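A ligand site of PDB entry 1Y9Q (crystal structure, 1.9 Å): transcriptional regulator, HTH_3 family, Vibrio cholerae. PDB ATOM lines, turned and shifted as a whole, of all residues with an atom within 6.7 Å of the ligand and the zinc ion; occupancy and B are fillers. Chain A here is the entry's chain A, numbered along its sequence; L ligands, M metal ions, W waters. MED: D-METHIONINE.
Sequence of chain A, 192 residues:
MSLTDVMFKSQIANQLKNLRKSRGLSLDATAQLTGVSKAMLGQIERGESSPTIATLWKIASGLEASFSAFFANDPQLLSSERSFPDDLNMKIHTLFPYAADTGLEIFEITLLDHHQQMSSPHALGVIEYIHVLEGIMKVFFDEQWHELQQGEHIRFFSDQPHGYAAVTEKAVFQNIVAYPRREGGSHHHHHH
Water W2 lies within hydrogen-bond range of the side-chain hydroxyl of Ser 119 (2.5 Å), the side-chain amide nitrogen of Gln 117 (2.7 Å) and an oxygen (OXT) of the ligand (2.7 Å).
Water W1 bridges the side-chain hydroxyl of Ser 119 (2.8 Å) and an oxygen (OXT) of the ligand (2.9 Å).
The nearest printed residue that does not touch the zinc ion is Ser 119 (4.2 Å).
Residues that only touch the ligand: Phe 107 (3.4 Å), Ile 109 (3.6 Å), Ile 92 (3.8 Å) and Ile 53 (3.9 Å).
Hydrophobic or aromatic side chains that line the ligand: Ile 53, Trp 57, Ile 92, Phe 107, Ile 109, His 122, His 162 and Tyr 164.
Within 4 Å of the ligand: Ile 53, Trp 57, Ile 92, Phe 107, Ile 109, Ser 119, His 122, Glu 128, His 162, Tyr 164 and Asn 175.
The nearest printed residue that does not touch the ligand is Val 177 (4.1 Å).
The zinc ion is bound by the side-chain carboxylate (OE2) of Glu 128 (2.1 Å), an oxygen (O) of the ligand (2.1 Å), a ring nitrogen (NE2) of His 122 (2.1 Å), the side-chain hydroxyl (OH) of Tyr 164 (2.2 Å), a nitrogen (N) of the ligand (2.2 Å) and a ring nitrogen (NE2) of His 162 (2.2 Å).
The side-chain hydroxyl (OG) of Ser 119 sits at hydrogen-bond distance from an oxygen (OXT) of the ligand (3.3 Å).
A nitrogen (N) of the ligand sits close to the side-chain amide nitrogen of Asn 175 (3.4 Å).
NE1 of Trp 57 lies close to SD of the ligand (3.3 Å).
The side-chain carboxylate (OE1) of Glu 128 sits close to the side-chain amide oxygen (OD1) of Asn 175, at 2.9 Å.
The backbone carbonyl oxygen (O) of Glu 128 lies within hydrogen-bond range of the backbone NH (N) of Phe 156 (2.9 Å).
The backbone NH (N) of His 122 is in hydrogen-bond range of the backbone carbonyl oxygen (O) of Ser 158 (2.9 Å).
O of Tyr 164 is in hydrogen-bond range of N of Gln 117 (2.6 Å).
The backbone carbonyl oxygen of His 162 sits at hydrogen-bond distance from the backbone NH of Ser 119 (2.7 Å).
The backbone NH (N) of Asn 175 sits at hydrogen-bond distance from the backbone carbonyl oxygen (O) of Phe 107 (2.8 Å).
The backbone carbonyl oxygen (O) of Phe 173 lies within hydrogen-bond range of the backbone NH (N) of Ile 109, 2.8 Å away.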
ATOM      1  N   ILE A  53     -26.839  27.102 -14.812  1.00  0.00           N
ATOM      2  CA  ILE A  53     -27.743  25.970 -14.941  1.00  0.00           C
ATOM      3  C   ILE A  53     -27.056  24.752 -14.337  1.00  0.00           C
ATOM      4  O   ILE A  53     -27.703  23.925 -13.696  1.00  0.00           O
ATOM      5  CB  ILE A  53     -28.057  25.689 -16.430  1.00  0.00           C
ATOM      6  CG1 ILE A  53     -28.898  26.846 -16.995  1.00  0.00           C
ATOM      7  CG2 ILE A  53     -28.791  24.355 -16.568  1.00  0.00           C
ATOM      8  CD1 ILE A  53     -29.288  26.691 -18.461  1.00  0.00           C
ATOM      9  N   ALA A  54     -25.745  24.647 -14.520  1.00  0.00           N
ATOM     10  CA  ALA A  54     -25.007  23.512 -13.994  1.00  0.00           C
ATOM     11  C   ALA A  54     -25.015  23.488 -12.462  1.00  0.00           C
ATOM     12  O   ALA A  54     -25.107  22.418 -11.850  1.00  0.00           O
ATOM     13  CB  ALA A  54     -23.572  23.525 -14.515  1.00  0.00           C
ATOM     14  N   TRP A  57     -28.475  22.304 -11.174  1.00  0.00           N
ATOM     15  CA  TRP A  57     -28.633  20.855 -11.208  1.00  0.00           C
ATOM     16  C   TRP A  57     -27.844  20.217 -10.070  1.00  0.00           C
ATOM     17  O   TRP A  57     -28.272  19.231  -9.466  1.00  0.00           O
ATOM     18  CB  TRP A  57     -28.169  20.279 -12.542  1.00  0.00           C
ATOM     19  CG  TRP A  57     -29.222  20.359 -13.616  1.00  0.00           C
ATOM     20  CD1 TRP A  57     -29.375  21.352 -14.544  1.00  0.00           C
ATOM     21  CD2 TRP A  57     -30.291  19.436 -13.839  1.00  0.00           C
ATOM     22  NE1 TRP A  57     -30.474  21.094 -15.325  1.00  0.00           N
ATOM     23  CE2 TRP A  57     -31.055  19.929 -14.910  1.00  0.00           C
ATOM     24  CE3 TRP A  57     -30.669  18.235 -13.224  1.00  0.00           C
ATOM     25  CZ2 TRP A  57     -32.194  19.262 -15.387  1.00  0.00           C
ATOM     26  CZ3 TRP A  57     -31.798  17.571 -13.698  1.00  0.00           C
ATOM     27  CH2 TRP A  57     -32.549  18.088 -14.765  1.00  0.00           C
ATOM     28  N   PHE A  67     -35.406  19.695 -11.187  1.00  0.00           N
ATOM     29  CA  PHE A  67     -34.956  21.009 -11.635  1.00  0.00           C
ATOM     30  C   PHE A  67     -36.195  21.918 -11.555  1.00  0.00           C
ATOM     31  O   PHE A  67     -36.115  23.085 -11.173  1.00  0.00           O
ATOM     32  CB  PHE A  67     -34.451  20.916 -13.085  1.00  0.00           C
ATOM     33  CG  PHE A  67     -33.953  22.215 -13.655  1.00  0.00           C
ATOM     34  CD1 PHE A  67     -32.672  22.682 -13.360  1.00  0.00           C
ATOM     35  CD2 PHE A  67     -34.761  22.979 -14.506  1.00  0.00           C
ATOM     36  CE1 PHE A  67     -32.206  23.880 -13.899  1.00  0.00           C
ATOM     37  CE2 PHE A  67     -34.293  24.178 -15.055  1.00  0.00           C
ATOM     38  CZ  PHE A  67     -33.009  24.625 -14.750  1.00  0.00           C
ATOM     39  N   MET A  90     -27.203  28.814 -24.381  1.00  0.00           N
ATOM     40  CA  MET A  90     -28.042  27.651 -24.130  1.00  0.00           C
ATOM     41  C   MET A  90     -29.411  28.150 -23.687  1.00  0.00           C
ATOM     42  O   MET A  90     -29.521  28.915 -22.741  1.00  0.00           O
ATOM     43  CB  MET A  90     -27.423  26.787 -23.031  1.00  0.00           C
ATOM     44  CG  MET A  90     -28.244  25.562 -22.662  1.00  0.00           C
ATOM     45  SD  MET A  90     -27.369  24.461 -21.341  1.00  0.00           S
ATOM     46  CE  MET A  90     -27.212  22.832 -22.360  1.00  0.00           C
ATOM     47  N   ILE A  92     -33.352  27.009 -22.581  1.00  0.00           N
ATOM     48  CA  ILE A  92     -34.178  25.906 -22.088  1.00  0.00           C
ATOM     49  C   ILE A  92     -35.671  26.154 -22.294  1.00  0.00           C
ATOM     50  O   ILE A  92     -36.211  27.155 -21.835  1.00  0.00           O
ATOM     51  CB  ILE A  92     -33.961  25.683 -20.570  1.00  0.00           C
ATOM     52  CG1 ILE A  92     -32.472  25.659 -20.237  1.00  0.00           C
ATOM     53  CG2 ILE A  92     -34.623  24.372 -20.138  1.00  0.00           C
ATOM     54  CD1 ILE A  92     -31.694  24.605 -20.953  1.00  0.00           C
ATOM     55  N   PHE A 107     -37.506  18.717 -21.519  1.00  0.00           N
ATOM     56  CA  PHE A 107     -37.043  19.988 -22.047  1.00  0.00           C
ATOM     57  C   PHE A 107     -36.659  19.923 -23.519  1.00  0.00           C
ATOM     58  O   PHE A 107     -36.357  18.852 -24.055  1.00  0.00           O
ATOM     59  CB  PHE A 107     -35.799  20.451 -21.307  1.00  0.00           C
ATOM     60  CG  PHE A 107     -35.913  20.394 -19.825  1.00  0.00           C
ATOM     61  CD1 PHE A 107     -36.502  21.428 -19.110  1.00  0.00           C
ATOM     62  CD2 PHE A 107     -35.398  19.301 -19.121  1.00  0.00           C
ATOM     63  CE1 PHE A 107     -36.582  21.386 -17.723  1.00  0.00           C
ATOM     64  CE2 PHE A 107     -35.476  19.249 -17.733  1.00  0.00           C
ATOM     65  CZ  PHE A 107     -36.062  20.293 -17.038  1.00  0.00           C
ATOM     66  N   GLU A 108     -36.682  21.083 -24.161  1.00  0.00           N
ATOM     67  CA  GLU A 108     -36.241  21.216 -25.542  1.00  0.00           C
ATOM     68  C   GLU A 108     -35.100  22.208 -25.381  1.00  0.00           C
ATOM     69  O   GLU A 108     -35.317  23.355 -24.998  1.00  0.00           O
ATOM     70  CB  GLU A 108     -37.342  21.803 -26.434  1.00  0.00           C
ATOM     71  CG  GLU A 108     -36.945  21.835 -27.901  1.00  0.00           C
ATOM     72  CD  GLU A 108     -38.117  22.036 -28.829  1.00  0.00           C
ATOM     73  OE1 GLU A 108     -39.021  21.180 -28.861  1.00  0.00           O
ATOM     74  OE2 GLU A 108     -38.121  23.062 -29.551  1.00  0.00           O
ATOM     75  N   ILE A 109     -33.878  21.761 -25.656  1.00  0.00           N
ATOM     76  CA  ILE A 109     -32.682  22.582 -25.473  1.00  0.00           C
ATOM     77  C   ILE A 109     -32.040  23.055 -26.773  1.00  0.00           C
ATOM     78  O   ILE A 109     -31.825  22.270 -27.690  1.00  0.00           O
ATOM     79  CB  ILE A 109     -31.597  21.796 -24.702  1.00  0.00           C
ATOM     80  CG1 ILE A 109     -32.188  21.179 -23.431  1.00  0.00           C
ATOM     81  CG2 ILE A 109     -30.427  22.712 -24.368  1.00  0.00           C
ATOM     82  CD1 ILE A 109     -32.905  22.156 -22.544  1.00  0.00           C
ATOM     83  N   GLN A 117     -21.585  22.133 -22.774  1.00  0.00           N
ATOM     84  CA  GLN A 117     -22.133  22.135 -21.420  1.00  0.00           C
ATOM     85  C   GLN A 117     -21.767  20.881 -20.635  1.00  0.00           C
ATOM     86  O   GLN A 117     -22.247  19.794 -20.938  1.00  0.00           O
ATOM     87  CB  GLN A 117     -23.667  22.244 -21.526  1.00  0.00           C
ATOM     88  CG  GLN A 117     -24.416  22.344 -20.216  1.00  0.00           C
ATOM     89  CD  GLN A 117     -24.188  23.665 -19.522  1.00  0.00           C
ATOM     90  OE1 GLN A 117     -23.891  24.676 -20.151  1.00  0.00           O
ATOM     91  NE2 GLN A 117     -24.328  23.664 -18.202  1.00  0.00           N
ATOM     92  N   MET A 118     -20.872  21.022 -19.653  1.00  0.00           N
ATOM     93  CA  MET A 118     -20.508  19.884 -18.824  1.00  0.00           C
ATOM     94  C   MET A 118     -21.374  19.917 -17.567  1.00  0.00           C
ATOM     95  O   MET A 118     -21.673  20.989 -17.041  1.00  0.00           O
ATOM     96  CB  MET A 118     -19.035  19.932 -18.432  1.00  0.00           C
ATOM     97  CG  MET A 118     -18.083  19.864 -19.614  1.00  0.00           C
ATOM     98  SD  MET A 118     -18.467  18.397 -20.799  1.00  0.00           S
ATOM     99  CE  MET A 118     -18.021  16.952 -19.590  1.00  0.00           C
ATOM    100  N   SER A 119     -21.768  18.746 -17.081  1.00  0.00           N
ATOM    101  CA  SER A 119     -22.620  18.654 -15.894  1.00  0.00           C
ATOM    102  C   SER A 119     -22.044  17.745 -14.829  1.00  0.00           C
ATOM    103  O   SER A 119     -21.292  16.823 -15.125  1.00  0.00           O
ATOM    104  CB  SER A 119     -24.001  18.102 -16.280  1.00  0.00           C
ATOM    105  OG  SER A 119     -24.661  18.934 -17.193  1.00  0.00           O
ATOM    106  N   SER A 120     -22.417  18.018 -13.579  1.00  0.00           N
ATOM    107  CA  SER A 120     -21.992  17.196 -12.449  1.00  0.00           C
ATOM    108  C   SER A 120     -22.989  16.036 -12.448  1.00  0.00           C
ATOM    109  O   SER A 120     -24.035  16.113 -13.075  1.00  0.00           O
ATOM    110  CB  SER A 120     -22.108  17.961 -11.132  1.00  0.00           C
ATOM    111  OG  SER A 120     -21.238  19.068 -11.085  1.00  0.00           O
ATOM    112  N   HIS A 122     -26.063  13.770 -11.756  1.00  0.00           N
ATOM    113  CA  HIS A 122     -27.387  14.100 -11.221  1.00  0.00           C
ATOM    114  C   HIS A 122     -27.576  13.053 -10.127  1.00  0.00           C
ATOM    115  O   HIS A 122     -26.684  12.233  -9.907  1.00  0.00           O
ATOM    116  CB  HIS A 122     -28.465  13.985 -12.304  1.00  0.00           C
ATOM    117  CG  HIS A 122     -28.312  14.980 -13.408  1.00  0.00           C
ATOM    118  ND1 HIS A 122     -27.830  16.259 -13.195  1.00  0.00           N
ATOM    119  CD2 HIS A 122     -28.590  14.896 -14.729  1.00  0.00           C
ATOM    120  CE1 HIS A 122     -27.824  16.919 -14.345  1.00  0.00           C
ATOM    121  NE2 HIS A 122     -28.278  16.123 -15.289  1.00  0.00           N
ATOM    122  N   GLU A 128     -31.236   9.902 -18.482  1.00  0.00           N
ATOM    123  CA  GLU A 128     -31.559  10.894 -19.498  1.00  0.00           C
ATOM    124  C   GLU A 128     -31.714  10.300 -20.876  1.00  0.00           C
ATOM    125  O   GLU A 128     -31.011   9.341 -21.228  1.00  0.00           O
ATOM    126  CB  GLU A 128     -30.492  11.987 -19.564  1.00  0.00           C
ATOM    127  CG  GLU A 128     -30.564  12.992 -18.428  1.00  0.00           C
ATOM    128  CD  GLU A 128     -29.609  14.149 -18.626  1.00  0.00           C
ATOM    129  OE1 GLU A 128     -29.557  14.699 -19.744  1.00  0.00           O
ATOM    130  OE2 GLU A 128     -28.900  14.497 -17.661  1.00  0.00           O
ATOM    131  N   PHE A 156     -28.752   7.465 -21.356  1.00  0.00           N
ATOM    132  CA  PHE A 156     -27.618   7.134 -20.502  1.00  0.00           C
ATOM    133  C   PHE A 156     -27.922   7.409 -19.036  1.00  0.00           C
ATOM    134  O   PHE A 156     -28.846   8.159 -18.717  1.00  0.00           O
ATOM    135  CB  PHE A 156     -26.390   7.948 -20.932  1.00  0.00           C
ATOM    136  CG  PHE A 156     -26.561   9.439 -20.770  1.00  0.00           C
ATOM    137  CD1 PHE A 156     -26.120  10.087 -19.624  1.00  0.00           C
ATOM    138  CD2 PHE A 156     -27.159  10.189 -21.782  1.00  0.00           C
ATOM    139  CE1 PHE A 156     -26.266  11.470 -19.476  1.00  0.00           C
ATOM    140  CE2 PHE A 156     -27.323  11.566 -21.639  1.00  0.00           C
ATOM    141  CZ  PHE A 156     -26.870  12.208 -20.490  1.00  0.00           C
ATOM    142  N   SER A 158     -27.364   9.317 -15.994  1.00  0.00           N
ATOM    143  CA  SER A 158     -26.831  10.644 -15.745  1.00  0.00           C
ATOM    144  C   SER A 158     -26.225  10.885 -14.374  1.00  0.00           C
ATOM    145  O   SER A 158     -25.783  12.002 -14.081  1.00  0.00           O
ATOM    146  CB  SER A 158     -27.909  11.701 -16.013  1.00  0.00           C
ATOM    147  OG  SER A 158     -28.960  11.623 -15.057  1.00  0.00           O
ATOM    148  N   HIS A 162     -21.261  14.118 -17.034  1.00  0.00           N
ATOM    149  CA  HIS A 162     -21.746  14.056 -18.411  1.00  0.00           C
ATOM    150  C   HIS A 162     -21.732  15.436 -19.029  1.00  0.00           C
ATOM    151  O   HIS A 162     -21.335  16.407 -18.377  1.00  0.00           O
ATOM    152  CB  HIS A 162     -23.159  13.431 -18.485  1.00  0.00           C
ATOM    153  CG  HIS A 162     -24.216  14.191 -17.735  1.00  0.00           C
ATOM    154  ND1 HIS A 162     -24.289  14.212 -16.366  1.00  0.00           N
ATOM    155  CD2 HIS A 162     -25.275  14.910 -18.179  1.00  0.00           C
ATOM    156  CE1 HIS A 162     -25.352  14.907 -15.992  1.00  0.00           C
ATOM    157  NE2 HIS A 162     -25.968  15.346 -17.076  1.00  0.00           N
ATOM    158  N   GLY A 163     -22.148  15.536 -20.281  1.00  0.00           N
ATOM    159  CA  GLY A 163     -22.147  16.839 -20.925  1.00  0.00           C
ATOM    160  C   GLY A 163     -22.790  16.827 -22.292  1.00  0.00           C
ATOM    161  O   GLY A 163     -23.095  15.765 -22.827  1.00  0.00           O
ATOM    162  N   TYR A 164     -22.989  18.018 -22.836  1.00  0.00           N
ATOM    163  CA  TYR A 164     -23.608  18.172 -24.153  1.00  0.00           C
ATOM    164  C   TYR A 164     -22.834  19.234 -24.921  1.00  0.00           C
ATOM    165  O   TYR A 164     -22.391  20.224 -24.340  1.00  0.00           O
ATOM    166  CB  TYR A 164     -25.048  18.644 -24.010  1.00  0.00           C
ATOM    167  CG  TYR A 164     -25.772  18.047 -22.828  1.00  0.00           C
ATOM    168  CD1 TYR A 164     -25.547  18.520 -21.536  1.00  0.00           C
ATOM    169  CD2 TYR A 164     -26.656  16.991 -22.992  1.00  0.00           C
ATOM    170  CE1 TYR A 164     -26.185  17.963 -20.433  1.00  0.00           C
ATOM    171  CE2 TYR A 164     -27.305  16.409 -21.903  1.00  0.00           C
ATOM    172  CZ  TYR A 164     -27.061  16.907 -20.626  1.00  0.00           C
ATOM    173  OH  TYR A 164     -27.692  16.329 -19.563  1.00  0.00           O
ATOM    174  N   PHE A 173     -32.143  19.842 -29.255  1.00  0.00           N
ATOM    175  CA  PHE A 173     -32.463  18.465 -28.897  1.00  0.00           C
ATOM    176  C   PHE A 173     -33.462  18.370 -27.761  1.00  0.00           C
ATOM    177  O   PHE A 173     -33.557  19.267 -26.933  1.00  0.00           O
ATOM    178  CB  PHE A 173     -31.179  17.700 -28.517  1.00  0.00           C
ATOM    179  CG  PHE A 173     -30.480  18.229 -27.281  1.00  0.00           C
ATOM    180  CD1 PHE A 173     -30.647  17.602 -26.051  1.00  0.00           C
ATOM    181  CD2 PHE A 173     -29.625  19.324 -27.363  1.00  0.00           C
ATOM    182  CE1 PHE A 173     -29.970  18.045 -24.916  1.00  0.00           C
ATOM    183  CE2 PHE A 173     -28.954  19.786 -26.230  1.00  0.00           C
ATOM    184  CZ  PHE A 173     -29.122  19.137 -25.010  1.00  0.00           C
ATOM    185  N   ASN A 175     -34.641  16.711 -24.355  1.00  0.00           N
ATOM    186  CA  ASN A 175     -33.988  16.044 -23.244  1.00  0.00           C
ATOM    187  C   ASN A 175     -35.048  15.592 -22.244  1.00  0.00           C
ATOM    188  O   ASN A 175     -35.760  16.416 -21.679  1.00  0.00           O
ATOM    189  CB  ASN A 175     -32.984  16.997 -22.582  1.00  0.00           C
ATOM    190  CG  ASN A 175     -32.222  16.363 -21.430  1.00  0.00           C
ATOM    191  OD1 ASN A 175     -31.886  15.176 -21.460  1.00  0.00           O
ATOM    192  ND2 ASN A 175     -31.920  17.163 -20.413  1.00  0.00           N
ATOM    193  N   VAL A 177     -35.602  13.865 -18.689  1.00  0.00           N
ATOM    194  CA  VAL A 177     -34.865  13.509 -17.468  1.00  0.00           C
ATOM    195  C   VAL A 177     -35.822  12.683 -16.601  1.00  0.00           C
ATOM    196  O   VAL A 177     -36.843  13.187 -16.136  1.00  0.00           O
ATOM    197  CB  VAL A 177     -34.413  14.772 -16.703  1.00  0.00           C
ATOM    198  CG1 VAL A 177     -33.652  14.373 -15.444  1.00  0.00           C
ATOM    199  CG2 VAL A 177     -33.537  15.637 -17.591  1.00  0.00           C
HETATM  200  N   MED L   1     -29.849  17.421 -17.730  1.00  0.00           N
HETATM  201  CA  MED L   1     -29.554  18.881 -17.813  1.00  0.00           C
HETATM  202  C   MED L   1     -28.076  19.152 -17.520  1.00  0.00           C
HETATM  203  O   MED L   1     -27.260  18.252 -17.249  1.00  0.00           O
HETATM  204  CB  MED L   1     -29.960  19.390 -19.223  1.00  0.00           C
HETATM  205  CG  MED L   1     -29.787  20.851 -19.568  1.00  0.00           C
HETATM  206  SD  MED L   1     -30.978  21.758 -18.531  1.00  0.00           S
HETATM  207  CE  MED L   1     -32.510  21.173 -19.113  1.00  0.00           C
HETATM  208  OXT MED L   1     -27.657  20.317 -17.543  1.00  0.00           O
HETATM  209 ZN    ZN M   1     -27.969  16.301 -17.369  1.00  0.00          ZN
HETATM  210  O   HOH W   1     -26.030  20.292 -15.099  1.00  0.00           O
HETATM  211  O   HOH W   2     -25.208  21.350 -17.202  1.00  0.00           O
